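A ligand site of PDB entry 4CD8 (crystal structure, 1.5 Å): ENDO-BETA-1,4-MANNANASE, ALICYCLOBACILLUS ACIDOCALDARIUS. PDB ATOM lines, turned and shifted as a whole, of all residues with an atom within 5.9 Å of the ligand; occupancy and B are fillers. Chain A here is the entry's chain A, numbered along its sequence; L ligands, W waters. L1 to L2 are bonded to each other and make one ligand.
An oxygen (O2) of LG2 L2 lies within hydrogen-bond range of the side-chain carboxylate (OE2) of Glu 282 (2.5 Å). A nitrogen (N2) of LIG L1 is in hydrogen-bond range of the side-chain carboxylate (OE2) of Glu 151, 2.5 Å away. O2 of LIG L1 lies within hydrogen-bond range of OE2 of Glu 231. The backbone carbonyl oxygen of Trp 245 is in hydrogen-bond range of an oxygen (O3) of LIG L1, at 2.7 Å. An oxygen (O2) of LIG L1 is in hydrogen-bond range of the guanidinium group (NH1) of Arg 104, 2.8 Å away. O3 of LIG L1 lies within hydrogen-bond range of OH of Tyr 299 (3.1 Å). The indole nitrogen (NE1) of Trp 281 sits at hydrogen-bond distance from an oxygen (O1) of LG2 L2 (3.1 Å). An oxygen (O6) of LG2 L2 lies within hydrogen-bond range of the side-chain amide nitrogen (ND2) of Asn 97.
The side-chain carboxylate of Glu 282 sits at hydrogen-bond distance from the indole nitrogen of Trp 281 (3.1 Å). The guanidinium group of Arg 104 is in salt-bridge range of the side-chain carboxylate of Glu 151, at 3.2 Å. OE2 of Glu 151 is in hydrogen-bond range of OG of Ser 201 (2.6 Å). The indole nitrogen of Trp 103 lies within hydrogen-bond range of the side-chain carboxylate of Glu 151. The side-chain sulfur (SG) of Cys 150 is in hydrogen-bond range of the side-chain carboxylate (OE2) of Glu 231, 3.4 Å away. The side-chain carboxylate (OE2) of Glu 231 is in salt-bridge range of the side-chain amino group (NZ) of Lys 93 (2.8 Å). O of Trp 245 sits close to OH of Tyr 299 (3.2 Å). The backbone NH (N) of Asp 246 is in hydrogen-bond range of the side-chain hydroxyl (OH) of Tyr 299, at 3.4 Å.
Residues that only touch the ligand: Tyr 247, Tyr 203, Phe 20 and Val 21. Hydrophobic or aromatic side chains within 4 Å of the ligand: Phe 20, Val 21, Tyr 203, Tyr 247, Trp 281 and Tyr 299. Of the 20 residues printed, 12 come within 4 Å of the ligand.
Water W1 lies within hydrogen-bond range of the side-chain carboxylate of Glu 151, a nitrogen (N2) of LIG L1, the indole nitrogen of Trp 103 and the guanidinium group of Arg 104.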
ATOM      1  N   PHE A  20      23.246   7.000 -34.246  1.00  0.00           N
ATOM      2  CA  PHE A  20      23.047   5.589 -33.828  1.00  0.00           C
ATOM      3  C   PHE A  20      21.795   5.516 -32.960  1.00  0.00           C
ATOM      4  O   PHE A  20      21.575   6.405 -32.148  1.00  0.00           O
ATOM      5  CB  PHE A  20      24.272   5.114 -33.039  1.00  0.00           C
ATOM      6  CG  PHE A  20      24.486   3.623 -33.043  1.00  0.00           C
ATOM      7  CD1 PHE A  20      24.709   2.959 -34.247  1.00  0.00           C
ATOM      8  CD2 PHE A  20      24.519   2.900 -31.854  1.00  0.00           C
ATOM      9  CE1 PHE A  20      24.952   1.626 -34.261  1.00  0.00           C
ATOM     10  CE2 PHE A  20      24.774   1.536 -31.871  1.00  0.00           C
ATOM     11  CZ  PHE A  20      24.996   0.895 -33.076  1.00  0.00           C
ATOM     12  N   VAL A  21      20.975   4.485 -33.091  1.00  0.00           N
ATOM     13  CA  VAL A  21      21.106   3.257 -33.884  1.00  0.00           C
ATOM     14  C   VAL A  21      20.531   3.339 -35.287  1.00  0.00           C
ATOM     15  O   VAL A  21      20.413   2.322 -35.988  1.00  0.00           O
ATOM     16  CB  VAL A  21      20.388   2.060 -33.176  1.00  0.00           C
ATOM     17  CG1 VAL A  21      20.988   1.807 -31.822  1.00  0.00           C
ATOM     18  CG2 VAL A  21      18.877   2.265 -33.050  1.00  0.00           C
ATOM     19  N   LYS A  93      28.782   3.426 -41.565  1.00  0.00           N
ATOM     20  CA  LYS A  93      29.029   2.337 -40.649  1.00  0.00           C
ATOM     21  C   LYS A  93      27.767   1.565 -40.342  1.00  0.00           C
ATOM     22  O   LYS A  93      27.072   1.843 -39.335  1.00  0.00           O
ATOM     23  CB  LYS A  93      29.672   2.814 -39.356  1.00  0.00           C
ATOM     24  CG  LYS A  93      30.025   1.719 -38.361  1.00  0.00           C
ATOM     25  CD  LYS A  93      30.722   2.317 -37.168  1.00  0.00           C
ATOM     26  CE  LYS A  93      30.601   1.496 -35.895  1.00  0.00           C
ATOM     27  NZ  LYS A  93      31.504   2.061 -34.878  1.00  0.00           N
ATOM     28  N   THR A  95      26.152  -1.757 -38.849  1.00  0.00           N
ATOM     29  CA  THR A  95      26.530  -2.870 -38.043  1.00  0.00           C
ATOM     30  C   THR A  95      25.280  -3.662 -37.652  1.00  0.00           C
ATOM     31  O   THR A  95      24.227  -3.464 -38.243  1.00  0.00           O
ATOM     32  CB  THR A  95      27.360  -2.419 -36.831  1.00  0.00           C
ATOM     33  OG1 THR A  95      27.886  -3.566 -36.174  1.00  0.00           O
ATOM     34  CG2 THR A  95      26.506  -1.629 -35.849  1.00  0.00           C
ATOM     35  N   ASN A  97      22.968  -5.361 -34.255  1.00  0.00           N
ATOM     36  CA  ASN A  97      22.673  -5.625 -32.852  1.00  0.00           C
ATOM     37  C   ASN A  97      21.751  -6.828 -32.761  1.00  0.00           C
ATOM     38  O   ASN A  97      21.128  -7.205 -33.736  1.00  0.00           O
ATOM     39  CB  ASN A  97      21.971  -4.419 -32.223  1.00  0.00           C
ATOM     40  CG  ASN A  97      22.948  -3.278 -31.947  1.00  0.00           C
ATOM     41  OD1 ASN A  97      24.165  -3.488 -31.958  1.00  0.00           O
ATOM     42  ND2 ASN A  97      22.416  -2.067 -31.714  1.00  0.00           N
ATOM     43  N   TRP A 103      25.534  -8.754 -27.070  1.00  0.00           N
ATOM     44  CA  TRP A 103      26.522  -7.921 -27.753  1.00  0.00           C
ATOM     45  C   TRP A 103      26.918  -8.593 -29.039  1.00  0.00           C
ATOM     46  O   TRP A 103      27.108  -9.814 -29.091  1.00  0.00           O
ATOM     47  CB  TRP A 103      27.704  -7.687 -26.842  1.00  0.00           C
ATOM     48  CG  TRP A 103      28.918  -7.039 -27.470  1.00  0.00           C
ATOM     49  CD1 TRP A 103      28.970  -5.868 -28.197  1.00  0.00           C
ATOM     50  CD2 TRP A 103      30.254  -7.528 -27.408  1.00  0.00           C
ATOM     51  NE1 TRP A 103      30.275  -5.616 -28.582  1.00  0.00           N
ATOM     52  CE2 TRP A 103      31.081  -6.612 -28.095  1.00  0.00           C
ATOM     53  CE3 TRP A 103      30.838  -8.638 -26.805  1.00  0.00           C
ATOM     54  CZ2 TRP A 103      32.446  -6.810 -28.227  1.00  0.00           C
ATOM     55  CZ3 TRP A 103      32.171  -8.811 -26.927  1.00  0.00           C
ATOM     56  CH2 TRP A 103      32.969  -7.901 -27.629  1.00  0.00           C
ATOM     57  N   ARG A 104      27.051  -7.764 -30.073  1.00  0.00           N
ATOM     58  CA  ARG A 104      27.385  -8.284 -31.404  1.00  0.00           C
ATOM     59  C   ARG A 104      28.680  -9.078 -31.430  1.00  0.00           C
ATOM     60  O   ARG A 104      28.850  -9.938 -32.264  1.00  0.00           O
ATOM     61  CB  ARG A 104      27.407  -7.141 -32.403  1.00  0.00           C
ATOM     62  CG  ARG A 104      28.537  -6.122 -32.244  1.00  0.00           C
ATOM     63  CD  ARG A 104      28.321  -4.933 -33.141  1.00  0.00           C
ATOM     64  NE  ARG A 104      27.336  -3.969 -32.687  1.00  0.00           N
ATOM     65  CZ  ARG A 104      27.587  -2.860 -31.979  1.00  0.00           C
ATOM     66  NH1 ARG A 104      28.819  -2.494 -31.626  1.00  0.00           N
ATOM     67  NH2 ARG A 104      26.572  -2.059 -31.670  1.00  0.00           N
ATOM     68  N   CYS A 150      32.160  -3.957 -36.912  1.00  0.00           N
ATOM     69  CA  CYS A 150      32.325  -3.323 -35.629  1.00  0.00           C
ATOM     70  C   CYS A 150      32.304  -4.396 -34.543  1.00  0.00           C
ATOM     71  O   CYS A 150      31.264  -5.014 -34.336  1.00  0.00           O
ATOM     72  CB  CYS A 150      31.197  -2.306 -35.446  1.00  0.00           C
ATOM     73  SG  CYS A 150      31.245  -1.440 -33.895  1.00  0.00           S
ATOM     74  N   GLU A 151      33.420  -4.561 -33.846  1.00  0.00           N
ATOM     75  CA  GLU A 151      33.477  -5.311 -32.578  1.00  0.00           C
ATOM     76  C   GLU A 151      33.080  -6.770 -32.686  1.00  0.00           C
ATOM     77  O   GLU A 151      32.521  -7.334 -31.737  1.00  0.00           O
ATOM     78  CB  GLU A 151      32.609  -4.631 -31.512  1.00  0.00           C
ATOM     79  CG  GLU A 151      33.166  -3.298 -31.074  1.00  0.00           C
ATOM     80  CD  GLU A 151      32.197  -2.474 -30.265  1.00  0.00           C
ATOM     81  OE1 GLU A 151      31.258  -3.058 -29.700  1.00  0.00           O
ATOM     82  OE2 GLU A 151      32.396  -1.258 -30.189  1.00  0.00           O
ATOM     83  N   ASN A 182      37.087  -4.469 -31.440  1.00  0.00           N
ATOM     84  CA  ASN A 182      36.943  -4.019 -30.045  1.00  0.00           C
ATOM     85  C   ASN A 182      38.284  -3.652 -29.398  1.00  0.00           C
ATOM     86  O   ASN A 182      39.327  -4.142 -29.788  1.00  0.00           O
ATOM     87  CB  ASN A 182      36.299  -5.121 -29.261  1.00  0.00           C
ATOM     88  CG  ASN A 182      35.641  -4.617 -27.986  1.00  0.00           C
ATOM     89  OD1 ASN A 182      35.251  -3.463 -27.895  1.00  0.00           O
ATOM     90  ND2 ASN A 182      35.525  -5.501 -27.021  1.00  0.00           N
ATOM     91  N   SER A 201      37.472   0.277 -31.186  1.00  0.00           N
ATOM     92  CA  SER A 201      36.566   0.903 -30.216  1.00  0.00           C
ATOM     93  C   SER A 201      37.374   1.042 -28.959  1.00  0.00           C
ATOM     94  O   SER A 201      37.404   0.146 -28.146  1.00  0.00           O
ATOM     95  CB  SER A 201      35.330   0.026 -29.997  1.00  0.00           C
ATOM     96  OG  SER A 201      34.491   0.047 -31.141  1.00  0.00           O
ATOM     97  N   TYR A 203      37.730   2.092 -25.987  1.00  0.00           N
ATOM     98  CA  TYR A 203      37.162   2.408 -24.666  1.00  0.00           C
ATOM     99  C   TYR A 203      38.070   1.907 -23.530  1.00  0.00           C
ATOM    100  O   TYR A 203      37.683   1.073 -22.711  1.00  0.00           O
ATOM    101  CB  TYR A 203      35.767   1.789 -24.562  1.00  0.00           C
ATOM    102  CG  TYR A 203      34.770   2.349 -25.545  1.00  0.00           C
ATOM    103  CD1 TYR A 203      34.185   3.592 -25.351  1.00  0.00           C
ATOM    104  CD2 TYR A 203      34.374   1.634 -26.650  1.00  0.00           C
ATOM    105  CE1 TYR A 203      33.255   4.114 -26.240  1.00  0.00           C
ATOM    106  CE2 TYR A 203      33.448   2.124 -27.535  1.00  0.00           C
ATOM    107  CZ  TYR A 203      32.886   3.369 -27.331  1.00  0.00           C
ATOM    108  OH  TYR A 203      31.960   3.900 -28.201  1.00  0.00           O
ATOM    109  N   GLU A 231      35.653   4.217 -32.639  1.00  0.00           N
ATOM    110  CA  GLU A 231      34.841   4.734 -31.547  1.00  0.00           C
ATOM    111  C   GLU A 231      35.740   5.040 -30.367  1.00  0.00           C
ATOM    112  O   GLU A 231      36.633   4.249 -30.032  1.00  0.00           O
ATOM    113  CB  GLU A 231      33.816   3.715 -31.033  1.00  0.00           C
ATOM    114  CG  GLU A 231      32.937   3.007 -32.057  1.00  0.00           C
ATOM    115  CD  GLU A 231      31.832   2.171 -31.435  1.00  0.00           C
ATOM    116  OE1 GLU A 231      31.638   2.268 -30.210  1.00  0.00           O
ATOM    117  OE2 GLU A 231      31.156   1.454 -32.198  1.00  0.00           O
ATOM    118  N   PRO A 244      34.422   2.956 -19.724  1.00  0.00           N
ATOM    119  CA  PRO A 244      33.866   3.941 -20.641  1.00  0.00           C
ATOM    120  C   PRO A 244      32.954   3.369 -21.724  1.00  0.00           C
ATOM    121  O   PRO A 244      32.148   4.095 -22.286  1.00  0.00           O
ATOM    122  CB  PRO A 244      35.091   4.622 -21.257  1.00  0.00           C
ATOM    123  CG  PRO A 244      36.251   3.772 -20.879  1.00  0.00           C
ATOM    124  CD  PRO A 244      35.885   3.057 -19.611  1.00  0.00           C
ATOM    125  N   TRP A 245      33.062   2.059 -21.946  1.00  0.00           N
ATOM    126  CA  TRP A 245      32.237   1.338 -22.915  1.00  0.00           C
ATOM    127  C   TRP A 245      30.794   1.145 -22.441  1.00  0.00           C
ATOM    128  O   TRP A 245      29.943   0.759 -23.234  1.00  0.00           O
ATOM    129  CB  TRP A 245      32.856  -0.062 -23.163  1.00  0.00           C
ATOM    130  CG  TRP A 245      32.963  -0.846 -21.886  1.00  0.00           C
ATOM    131  CD1 TRP A 245      31.945  -1.530 -21.261  1.00  0.00           C
ATOM    132  CD2 TRP A 245      34.100  -0.938 -21.026  1.00  0.00           C
ATOM    133  NE1 TRP A 245      32.394  -2.050 -20.077  1.00  0.00           N
ATOM    134  CE2 TRP A 245      33.708  -1.708 -19.898  1.00  0.00           C
ATOM    135  CE3 TRP A 245      35.411  -0.451 -21.088  1.00  0.00           C
ATOM    136  CZ2 TRP A 245      34.600  -2.025 -18.860  1.00  0.00           C
ATOM    137  CZ3 TRP A 245      36.284  -0.756 -20.057  1.00  0.00           C
ATOM    138  CH2 TRP A 245      35.887  -1.541 -18.962  1.00  0.00           C
ATOM    139  N   ASP A 246      30.520   1.361 -21.152  1.00  0.00           N
ATOM    140  CA  ASP A 246      29.235   0.950 -20.579  1.00  0.00           C
ATOM    141  C   ASP A 246      28.209   2.070 -20.675  1.00  0.00           C
ATOM    142  O   ASP A 246      28.283   3.050 -19.934  1.00  0.00           O
ATOM    143  CB  ASP A 246      29.441   0.535 -19.113  1.00  0.00           C
ATOM    144  CG  ASP A 246      28.222  -0.164 -18.520  1.00  0.00           C
ATOM    145  OD1 ASP A 246      27.100  -0.057 -19.068  1.00  0.00           O
ATOM    146  OD2 ASP A 246      28.393  -0.836 -17.491  1.00  0.00           O
ATOM    147  N   TYR A 247      27.234   1.913 -21.576  1.00  0.00           N
ATOM    148  CA  TYR A 247      26.164   2.916 -21.746  1.00  0.00           C
ATOM    149  C   TYR A 247      25.007   2.798 -20.742  1.00  0.00           C
ATOM    150  O   TYR A 247      24.061   3.573 -20.803  1.00  0.00           O
ATOM    151  CB  TYR A 247      25.576   2.908 -23.162  1.00  0.00           C
ATOM    152  CG  TYR A 247      24.800   1.678 -23.579  1.00  0.00           C
ATOM    153  CD1 TYR A 247      25.472   0.597 -24.151  1.00  0.00           C
ATOM    154  CD2 TYR A 247      23.427   1.632 -23.501  1.00  0.00           C
ATOM    155  CE1 TYR A 247      24.802  -0.517 -24.587  1.00  0.00           C
ATOM    156  CE2 TYR A 247      22.723   0.503 -23.941  1.00  0.00           C
ATOM    157  CZ  TYR A 247      23.437  -0.562 -24.486  1.00  0.00           C
ATOM    158  OH  TYR A 247      22.818  -1.697 -24.941  1.00  0.00           O
ATOM    159  N   TRP A 281      32.592   9.021 -30.035  1.00  0.00           N
ATOM    160  CA  TRP A 281      31.317   8.372 -29.782  1.00  0.00           C
ATOM    161  C   TRP A 281      30.649   9.174 -28.670  1.00  0.00           C
ATOM    162  O   TRP A 281      31.236   9.266 -27.594  1.00  0.00           O
ATOM    163  CB  TRP A 281      31.542   6.938 -29.277  1.00  0.00           C
ATOM    164  CG  TRP A 281      30.201   6.212 -29.205  1.00  0.00           C
ATOM    165  CD1 TRP A 281      29.315   6.200 -28.181  1.00  0.00           C
ATOM    166  CD2 TRP A 281      29.583   5.488 -30.278  1.00  0.00           C
ATOM    167  NE1 TRP A 281      28.218   5.482 -28.515  1.00  0.00           N
ATOM    168  CE2 TRP A 281      28.336   5.039 -29.809  1.00  0.00           C
ATOM    169  CE3 TRP A 281      29.983   5.156 -31.583  1.00  0.00           C
ATOM    170  CZ2 TRP A 281      27.477   4.283 -30.571  1.00  0.00           C
ATOM    171  CZ3 TRP A 281      29.150   4.373 -32.349  1.00  0.00           C
ATOM    172  CH2 TRP A 281      27.892   3.956 -31.847  1.00  0.00           C
ATOM    173  N   GLU A 282      29.483   9.787 -28.885  1.00  0.00           N
ATOM    174  CA  GLU A 282      28.701   9.843 -30.113  1.00  0.00           C
ATOM    175  C   GLU A 282      27.811  11.131 -30.041  1.00  0.00           C
ATOM    176  O   GLU A 282      27.823  11.897 -29.053  1.00  0.00           O
ATOM    177  CB  GLU A 282      27.753   8.632 -30.248  1.00  0.00           C
ATOM    178  CG  GLU A 282      26.827   8.516 -29.038  1.00  0.00           C
ATOM    179  CD  GLU A 282      25.776   7.423 -29.119  1.00  0.00           C
ATOM    180  OE1 GLU A 282      25.242   7.172 -30.215  1.00  0.00           O
ATOM    181  OE2 GLU A 282      25.447   6.815 -28.053  1.00  0.00           O
ATOM    182  N   TYR A 299      26.910   9.910 -23.880  1.00  0.00           N
ATOM    183  CA  TYR A 299      28.246  10.091 -24.448  1.00  0.00           C
ATOM    184  C   TYR A 299      28.440  11.435 -25.114  1.00  0.00           C
ATOM    185  O   TYR A 299      29.591  11.832 -25.383  1.00  0.00           O
ATOM    186  CB  TYR A 299      28.535   9.005 -25.478  1.00  0.00           C
ATOM    187  CG  TYR A 299      28.855   7.673 -24.875  1.00  0.00           C
ATOM    188  CD1 TYR A 299      27.842   6.792 -24.517  1.00  0.00           C
ATOM    189  CD2 TYR A 299      30.173   7.272 -24.687  1.00  0.00           C
ATOM    190  CE1 TYR A 299      28.145   5.555 -23.972  1.00  0.00           C
ATOM    191  CE2 TYR A 299      30.487   6.026 -24.147  1.00  0.00           C
ATOM    192  CZ  TYR A 299      29.472   5.173 -23.776  1.00  0.00           C
ATOM    193  OH  TYR A 299      29.775   3.954 -23.246  1.00  0.00           O
HETATM  194  C1  LIG L   1      29.848   0.741 -28.655  1.00  0.00           C
HETATM  195  N1  LIG L   1      29.684   1.326 -27.477  1.00  0.00           N
HETATM  196  C2  LIG L   1      27.521   1.104 -29.321  1.00  0.00           C
HETATM  197  C3  LIG L   1      27.378   1.768 -27.937  1.00  0.00           C
HETATM  198  C4  LIG L   1      28.685   2.385 -27.406  1.00  0.00           C
HETATM  199  C5  LIG L   1      28.624   2.938 -25.982  1.00  0.00           C
HETATM  200  C6  LIG L   1      31.231  -0.178 -27.231  1.00  0.00           C
HETATM  201  C7  LIG L   1      30.523   0.810 -26.567  1.00  0.00           C
HETATM  202  N2  LIG L   1      30.810  -0.184 -28.522  1.00  0.00           N
HETATM  203  O1  LIG L   1      27.100  -0.254 -29.324  1.00  0.00           O
HETATM  204  O2  LIG L   1      29.104   0.246 -30.931  1.00  0.00           O
HETATM  205  C8  LIG L   1      28.979   1.136 -29.810  1.00  0.00           C
HETATM  206  O3  LIG L   1      28.238   1.948 -25.007  1.00  0.00           O
HETATM  207  C1  LG2 L   2      25.219   2.567 -27.504  1.00  0.00           C
HETATM  208  C2  LG2 L   2      24.367   3.816 -27.309  1.00  0.00           C
HETATM  209  C3  LG2 L   2      22.941   3.378 -26.948  1.00  0.00           C
HETATM  210  C4  LG2 L   2      22.469   2.344 -27.965  1.00  0.00           C
HETATM  211  C5  LG2 L   2      23.424   1.162 -28.040  1.00  0.00           C
HETATM  212  C6  LG2 L   2      22.942   0.015 -28.925  1.00  0.00           C
HETATM  213  O1  LG2 L   2      26.520   2.950 -27.876  1.00  0.00           O
HETATM  214  O2  LG2 L   2      24.219   4.629 -28.441  1.00  0.00           O
HETATM  215  O3  LG2 L   2      22.053   4.500 -26.891  1.00  0.00           O
HETATM  216  O4  LG2 L   2      21.223   1.896 -27.466  1.00  0.00           O
HETATM  217  O5  LG2 L   2      24.677   1.696 -28.502  1.00  0.00           O
HETATM  218  O6  LG2 L   2      24.034  -0.839 -29.299  1.00  0.00           O
HETATM  219  O   HOH W   1      29.167  -2.547 -28.265  1.00  0.00           O
HETATM  220  O   HOH W   2      33.622  -2.303 -26.142  1.00  0.00           O
